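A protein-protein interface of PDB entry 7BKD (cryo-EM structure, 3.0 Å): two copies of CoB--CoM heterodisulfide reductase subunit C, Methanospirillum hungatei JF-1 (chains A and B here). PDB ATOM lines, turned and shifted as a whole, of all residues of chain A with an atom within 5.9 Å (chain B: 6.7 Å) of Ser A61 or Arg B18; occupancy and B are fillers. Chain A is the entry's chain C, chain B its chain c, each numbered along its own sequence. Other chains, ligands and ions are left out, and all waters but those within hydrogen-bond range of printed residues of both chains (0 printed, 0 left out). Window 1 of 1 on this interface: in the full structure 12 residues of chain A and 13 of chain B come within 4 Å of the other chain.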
ATOM      1  N   SER A  56     -22.048   8.898   7.348  1.00  0.00           N
ATOM      2  CA  SER A  56     -20.646   9.034   7.721  1.00  0.00           C
ATOM      3  C   SER A  56     -20.195  10.483   7.831  1.00  0.00           C
ATOM      4  O   SER A  56     -19.277  10.777   8.604  1.00  0.00           O
ATOM      5  CB  SER A  56     -19.756   8.309   6.709  1.00  0.00           C
ATOM      6  OG  SER A  56     -19.854   6.905   6.853  1.00  0.00           O
ATOM      7  N   ALA A  57     -20.813  11.387   7.075  1.00  0.00           N
ATOM      8  CA  ALA A  57     -20.394  12.786   7.086  1.00  0.00           C
ATOM      9  C   ALA A  57     -20.473  13.464   8.455  1.00  0.00           C
ATOM     10  O   ALA A  57     -19.535  14.206   8.790  1.00  0.00           O
ATOM     11  CB  ALA A  57     -21.206  13.572   6.050  1.00  0.00           C
ATOM     12  N   PRO A  58     -21.522  13.288   9.268  1.00  0.00           N
ATOM     13  CA  PRO A  58     -21.607  14.063  10.518  1.00  0.00           C
ATOM     14  C   PRO A  58     -20.523  13.751  11.537  1.00  0.00           C
ATOM     15  O   PRO A  58     -20.349  14.533  12.477  1.00  0.00           O
ATOM     16  CB  PRO A  58     -22.994  13.696  11.068  1.00  0.00           C
ATOM     17  CG  PRO A  58     -23.730  13.141   9.928  1.00  0.00           C
ATOM     18  CD  PRO A  58     -22.726  12.461   9.081  1.00  0.00           C
ATOM     19  N   ARG A  59     -19.802  12.637  11.405  1.00  0.00           N
ATOM     20  CA  ARG A  59     -18.875  12.199  12.442  1.00  0.00           C
ATOM     21  C   ARG A  59     -17.452  12.030  11.924  1.00  0.00           C
ATOM     22  O   ARG A  59     -16.631  11.392  12.586  1.00  0.00           O
ATOM     23  CB  ARG A  59     -19.363  10.893  13.070  1.00  0.00           C
ATOM     24  CG  ARG A  59     -19.552   9.774  12.069  1.00  0.00           C
ATOM     25  CD  ARG A  59     -20.310   8.609  12.658  1.00  0.00           C
ATOM     26  NE  ARG A  59     -21.376   9.026  13.563  1.00  0.00           N
ATOM     27  CZ  ARG A  59     -22.583   9.420  13.172  1.00  0.00           C
ATOM     28  NH1 ARG A  59     -22.889   9.459  11.886  1.00  0.00           N
ATOM     29  NH2 ARG A  59     -23.485   9.775  14.072  1.00  0.00           N
ATOM     30  N   SER A  60     -17.138  12.590  10.765  1.00  0.00           N
ATOM     31  CA  SER A  60     -15.821  12.426  10.167  1.00  0.00           C
ATOM     32  C   SER A  60     -15.610  13.558   9.171  1.00  0.00           C
ATOM     33  O   SER A  60     -16.407  14.498   9.099  1.00  0.00           O
ATOM     34  CB  SER A  60     -15.688  11.047   9.513  1.00  0.00           C
ATOM     35  OG  SER A  60     -16.502  10.949   8.362  1.00  0.00           O
ATOM     36  N   SER A  61     -14.530  13.469   8.402  1.00  0.00           N
ATOM     37  CA  SER A  61     -14.246  14.417   7.336  1.00  0.00           C
ATOM     38  C   SER A  61     -14.683  13.908   5.966  1.00  0.00           C
ATOM     39  O   SER A  61     -14.431  14.577   4.960  1.00  0.00           O
ATOM     40  CB  SER A  61     -12.756  14.759   7.321  1.00  0.00           C
ATOM     41  OG  SER A  61     -11.972  13.625   7.007  1.00  0.00           O
ATOM     42  N   TYR A  62     -15.334  12.748   5.908  1.00  0.00           N
ATOM     43  CA  TYR A  62     -15.770  12.177   4.640  1.00  0.00           C
ATOM     44  C   TYR A  62     -16.849  13.043   4.001  1.00  0.00           C
ATOM     45  O   TYR A  62     -17.862  13.359   4.629  1.00  0.00           O
ATOM     46  CB  TYR A  62     -16.288  10.756   4.863  1.00  0.00           C
ATOM     47  CG  TYR A  62     -16.898  10.100   3.645  1.00  0.00           C
ATOM     48  CD1 TYR A  62     -16.153   9.895   2.496  1.00  0.00           C
ATOM     49  CD2 TYR A  62     -18.219   9.675   3.649  1.00  0.00           C
ATOM     50  CE1 TYR A  62     -16.702   9.293   1.387  1.00  0.00           C
ATOM     51  CE2 TYR A  62     -18.777   9.071   2.543  1.00  0.00           C
ATOM     52  CZ  TYR A  62     -18.016   8.884   1.415  1.00  0.00           C
ATOM     53  OH  TYR A  62     -18.568   8.284   0.312  1.00  0.00           O
ATOM     54  N   ARG A  63     -16.622  13.432   2.749  1.00  0.00           N
ATOM     55  CA  ARG A  63     -17.576  14.215   1.969  1.00  0.00           C
ATOM     56  C   ARG A  63     -17.686  13.570   0.596  1.00  0.00           C
ATOM     57  O   ARG A  63     -16.747  13.642  -0.201  1.00  0.00           O
ATOM     58  CB  ARG A  63     -17.139  15.675   1.845  1.00  0.00           C
ATOM     59  CG  ARG A  63     -16.890  16.382   3.159  1.00  0.00           C
ATOM     60  CD  ARG A  63     -18.187  16.723   3.855  1.00  0.00           C
ATOM     61  NE  ARG A  63     -17.948  17.390   5.128  1.00  0.00           N
ATOM     62  CZ  ARG A  63     -17.852  16.759   6.294  1.00  0.00           C
ATOM     63  NH1 ARG A  63     -17.975  15.443   6.348  1.00  0.00           N
ATOM     64  NH2 ARG A  63     -17.629  17.446   7.404  1.00  0.00           N
ATOM     65  N   LEU A  66     -17.248  16.029  -2.359  1.00  0.00           N
ATOM     66  CA  LEU A  66     -15.869  16.320  -2.739  1.00  0.00           C
ATOM     67  C   LEU A  66     -15.289  15.216  -3.611  1.00  0.00           C
ATOM     68  O   LEU A  66     -14.529  15.491  -4.543  1.00  0.00           O
ATOM     69  CB  LEU A  66     -14.991  16.536  -1.506  1.00  0.00           C
ATOM     70  CG  LEU A  66     -15.267  17.751  -0.627  1.00  0.00           C
ATOM     71  CD1 LEU A  66     -14.384  17.708   0.610  1.00  0.00           C
ATOM     72  CD2 LEU A  66     -15.035  19.029  -1.415  1.00  0.00           C
ATOM     73  N   ASP A  84     -10.345   8.881   4.003  1.00  0.00           N
ATOM     74  CA  ASP A  84     -11.806   8.894   4.039  1.00  0.00           C
ATOM     75  C   ASP A  84     -12.389   8.424   2.712  1.00  0.00           C
ATOM     76  O   ASP A  84     -13.317   9.013   2.174  1.00  0.00           O
ATOM     77  CB  ASP A  84     -12.315  10.286   4.389  1.00  0.00           C
ATOM     78  CG  ASP A  84     -11.653  10.861   5.621  1.00  0.00           C
ATOM     79  OD1 ASP A  84     -11.748  10.239   6.698  1.00  0.00           O
ATOM     80  OD2 ASP A  84     -11.048  11.948   5.517  1.00  0.00           O
ATOM     81  N   LEU A  87     -14.670   5.004   4.517  1.00  0.00           N
ATOM     82  CA  LEU A  87     -15.707   5.290   5.495  1.00  0.00           C
ATOM     83  C   LEU A  87     -17.110   5.204   4.910  1.00  0.00           C
ATOM     84  O   LEU A  87     -18.083   5.334   5.658  1.00  0.00           O
ATOM     85  CB  LEU A  87     -15.491   6.675   6.108  1.00  0.00           C
ATOM     86  CG  LEU A  87     -14.302   6.821   7.057  1.00  0.00           C
ATOM     87  CD1 LEU A  87     -14.161   8.264   7.488  1.00  0.00           C
ATOM     88  CD2 LEU A  87     -14.462   5.913   8.259  1.00  0.00           C
ATOM     89  N   ALA B   2     -20.189  11.147  16.559  1.00  0.00           N
ATOM     90  CA  ALA B   2     -21.030  12.322  16.740  1.00  0.00           C
ATOM     91  C   ALA B   2     -22.364  11.957  17.378  1.00  0.00           C
ATOM     92  O   ALA B   2     -23.299  12.756  17.372  1.00  0.00           O
ATOM     93  CB  ALA B   2     -21.254  13.020  15.408  1.00  0.00           C
ATOM     94  N   ASP B  12     -13.766  11.802  21.474  1.00  0.00           N
ATOM     95  CA  ASP B  12     -14.510  13.043  21.298  1.00  0.00           C
ATOM     96  C   ASP B  12     -13.908  13.900  20.195  1.00  0.00           C
ATOM     97  O   ASP B  12     -14.640  14.595  19.481  1.00  0.00           O
ATOM     98  CB  ASP B  12     -14.561  13.822  22.610  1.00  0.00           C
ATOM     99  CG  ASP B  12     -14.992  12.962  23.782  1.00  0.00           C
ATOM    100  OD1 ASP B  12     -15.954  12.182  23.625  1.00  0.00           O
ATOM    101  OD2 ASP B  12     -14.379  13.075  24.864  1.00  0.00           O
ATOM    102  N   LYS B  13     -12.585  13.867  20.038  1.00  0.00           N
ATOM    103  CA  LYS B  13     -11.961  14.591  18.937  1.00  0.00           C
ATOM    104  C   LYS B  13     -12.208  13.888  17.608  1.00  0.00           C
ATOM    105  O   LYS B  13     -12.444  14.544  16.586  1.00  0.00           O
ATOM    106  CB  LYS B  13     -10.462  14.744  19.197  1.00  0.00           C
ATOM    107  CG  LYS B  13      -9.694  15.401  18.065  1.00  0.00           C
ATOM    108  CD  LYS B  13      -8.282  15.760  18.498  1.00  0.00           C
ATOM    109  CE  LYS B  13      -7.467  16.304  17.336  1.00  0.00           C
ATOM    110  NZ  LYS B  13      -8.189  16.191  16.042  1.00  0.00           N
ATOM    111  N   LYS B  14     -12.162  12.555  17.603  1.00  0.00           N
ATOM    112  CA  LYS B  14     -12.314  11.798  16.367  1.00  0.00           C
ATOM    113  C   LYS B  14     -13.767  11.750  15.907  1.00  0.00           C
ATOM    114  O   LYS B  14     -14.029  11.720  14.700  1.00  0.00           O
ATOM    115  CB  LYS B  14     -11.731  10.397  16.570  1.00  0.00           C
ATOM    116  CG  LYS B  14     -11.627   9.500  15.345  1.00  0.00           C
ATOM    117  CD  LYS B  14     -12.840   8.628  15.140  1.00  0.00           C
ATOM    118  CE  LYS B  14     -12.638   7.705  13.953  1.00  0.00           C
ATOM    119  NZ  LYS B  14     -13.830   6.856  13.704  1.00  0.00           N
ATOM    120  N   LEU B  15     -14.716  11.764  16.840  1.00  0.00           N
ATOM    121  CA  LEU B  15     -16.142  11.742  16.539  1.00  0.00           C
ATOM    122  C   LEU B  15     -16.807  13.082  16.841  1.00  0.00           C
ATOM    123  O   LEU B  15     -17.943  13.134  17.312  1.00  0.00           O
ATOM    124  CB  LEU B  15     -16.846  10.629  17.311  1.00  0.00           C
ATOM    125  CG  LEU B  15     -16.312   9.204  17.179  1.00  0.00           C
ATOM    126  CD1 LEU B  15     -17.099   8.270  18.078  1.00  0.00           C
ATOM    127  CD2 LEU B  15     -16.378   8.744  15.735  1.00  0.00           C
ATOM    128  N   ALA B  16     -16.101  14.180  16.586  1.00  0.00           N
ATOM    129  CA  ALA B  16     -16.689  15.498  16.779  1.00  0.00           C
ATOM    130  C   ALA B  16     -17.870  15.693  15.838  1.00  0.00           C
ATOM    131  O   ALA B  16     -17.832  15.284  14.675  1.00  0.00           O
ATOM    132  CB  ALA B  16     -15.644  16.585  16.541  1.00  0.00           C
ATOM    133  N   ASP B  17     -18.932  16.310  16.347  1.00  0.00           N
ATOM    134  CA  ASP B  17     -20.104  16.565  15.522  1.00  0.00           C
ATOM    135  C   ASP B  17     -19.774  17.640  14.494  1.00  0.00           C
ATOM    136  O   ASP B  17     -19.475  18.782  14.852  1.00  0.00           O
ATOM    137  CB  ASP B  17     -21.285  16.991  16.387  1.00  0.00           C
ATOM    138  CG  ASP B  17     -22.620  16.780  15.694  1.00  0.00           C
ATOM    139  OD1 ASP B  17     -22.660  16.780  14.445  1.00  0.00           O
ATOM    140  OD2 ASP B  17     -23.636  16.618  16.401  1.00  0.00           O
ATOM    141  N   ARG B  18     -19.827  17.273  13.217  1.00  0.00           N
ATOM    142  CA  ARG B  18     -19.505  18.184  12.131  1.00  0.00           C
ATOM    143  C   ARG B  18     -20.713  18.950  11.606  1.00  0.00           C
ATOM    144  O   ARG B  18     -20.550  19.798  10.724  1.00  0.00           O
ATOM    145  CB  ARG B  18     -18.857  17.416  10.975  1.00  0.00           C
ATOM    146  CG  ARG B  18     -17.341  17.426  10.979  1.00  0.00           C
ATOM    147  CD  ARG B  18     -16.783  16.417  11.959  1.00  0.00           C
ATOM    148  NE  ARG B  18     -15.443  15.976  11.589  1.00  0.00           N
ATOM    149  CZ  ARG B  18     -14.768  15.029  12.229  1.00  0.00           C
ATOM    150  NH1 ARG B  18     -13.557  14.684  11.820  1.00  0.00           N
ATOM    151  NH2 ARG B  18     -15.307  14.422  13.276  1.00  0.00           N
ATOM    152  N   ARG B  19     -21.912  18.681  12.119  1.00  0.00           N
ATOM    153  CA  ARG B  19     -23.116  19.312  11.598  1.00  0.00           C
ATOM    154  C   ARG B  19     -23.318  20.691  12.208  1.00  0.00           C
ATOM    155  O   ARG B  19     -23.312  20.846  13.432  1.00  0.00           O
ATOM    156  CB  ARG B  19     -24.347  18.452  11.876  1.00  0.00           C
ATOM    157  CG  ARG B  19     -24.802  17.606  10.714  1.00  0.00           C
ATOM    158  CD  ARG B  19     -25.997  16.769  11.118  1.00  0.00           C
ATOM    159  NE  ARG B  19     -26.353  15.782  10.106  1.00  0.00           N
ATOM    160  CZ  ARG B  19     -26.901  14.606  10.384  1.00  0.00           C
ATOM    161  NH1 ARG B  19     -27.152  14.276  11.644  1.00  0.00           N
ATOM    162  NH2 ARG B  19     -27.192  13.760   9.410  1.00  0.00           N
ATOM    163  N   TYR B  20     -23.518  21.685  11.351  1.00  0.00           N
ATOM    164  CA  TYR B  20     -23.913  23.003  11.821  1.00  0.00           C
ATOM    165  C   TYR B  20     -25.339  22.942  12.351  1.00  0.00           C
ATOM    166  O   TYR B  20     -26.240  22.438  11.674  1.00  0.00           O
ATOM    167  CB  TYR B  20     -23.802  24.030  10.697  1.00  0.00           C
ATOM    168  CG  TYR B  20     -24.463  25.352  11.021  1.00  0.00           C
ATOM    169  CD1 TYR B  20     -23.809  26.307  11.784  1.00  0.00           C
ATOM    170  CD2 TYR B  20     -25.745  25.641  10.571  1.00  0.00           C
ATOM    171  CE1 TYR B  20     -24.408  27.510  12.087  1.00  0.00           C
ATOM    172  CE2 TYR B  20     -26.354  26.841  10.870  1.00  0.00           C
ATOM    173  CZ  TYR B  20     -25.680  27.773  11.629  1.00  0.00           C
ATOM    174  OH  TYR B  20     -26.278  28.974  11.929  1.00  0.00           O
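The backbone carbonyl oxygen of Pro A58 is in hydrogen-bond range of the backbone NH of Arg B18 (2.9 Å). The guanidinium group (NH2) of Arg B18 lies within hydrogen-bond range of the backbone carbonyl oxygen (O) of Arg A59. The backbone carbonyl oxygen of Ser A60 lies within hydrogen-bond range of the guanidinium group of Arg B18, 3.1 Å away. O of Pro A58 sits close to O of Ala B16. O of Lys B14 lies close to O of Arg A59 (3.4 Å).
The backbone carbonyl oxygen of Ser A56 lies within hydrogen-bond range of the side-chain hydroxyl of Ser A60 (2.8 Å). The backbone carbonyl oxygen of Ser A60 is in hydrogen-bond range of the guanidinium group of Arg A63 (3.3 Å). OG of Ser A61 lies within hydrogen-bond range of OD2 of Asp A84, at 2.4 Å. The backbone NH (N) of Ala B2 sits at hydrogen-bond distance from the backbone carbonyl oxygen (O) of Leu B15 (3.1 Å). The guanidinium group of Arg B18 lies within hydrogen-bond range of the backbone carbonyl oxygen of Lys B14 (3.3 Å). The backbone carbonyl oxygen of Ala B16 is in hydrogen-bond range of the guanidinium group of Arg B18, 3.0 Å away.
Ala A57 touches Arg B18. CB of Ala B2 touches O of Pro A58, 3.4 Å away. Pro A58 touches Asp B17 (O to CA, 3.7 Å). CG of Pro A58 touches CZ of Arg B19, 3.5 Å away. CB of Arg A59 touches N of Ala B2 (3.6 Å). Arg A59 touches Leu B15 (O to CA, 3.998 Å). Ala B16 touches Arg A59. Ser A61 touches Arg B18 (N to NH1, 3.8 Å). Arg A63 touches Arg B18 (NH2 to CG, 3.6 Å).
Of chain A, only Ala A57 (3.9 Å), Pro A58 (2.9 Å), Arg A59 (3.4 Å), Ser A60 (3.1 Å), Ser A61 (3.8 Å) and Arg A63 (3.6 Å) come within 4 Å of Arg B18. Of the printed residues of chain B, Ala A57 touches Arg B18. Of the printed residues of chain A, Ala B16 touches Pro A58 and Arg A59. Of the printed residues of chain A, Lys B14 touches Arg A59 (3.4 Å). The nearest printed residue of chain A that does not touch Arg B18 is Tyr A62 (6.5 Å). The nearest printed residue of chain A that does not touch Arg B19 is Ala A57 (6.1 Å).
Of the 11 printed residues of chain A, 6 touch a printed residue of chain B. Among the printed residues, no Asp or Glu carboxylate lies within 4 Å of a Lys or Arg side-chain nitrogen of the other chain.
No position is printed for both chains. Of the 14 pairs that touch across the chains among the printed residues, none has its exchanged pair printed and touching as well.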
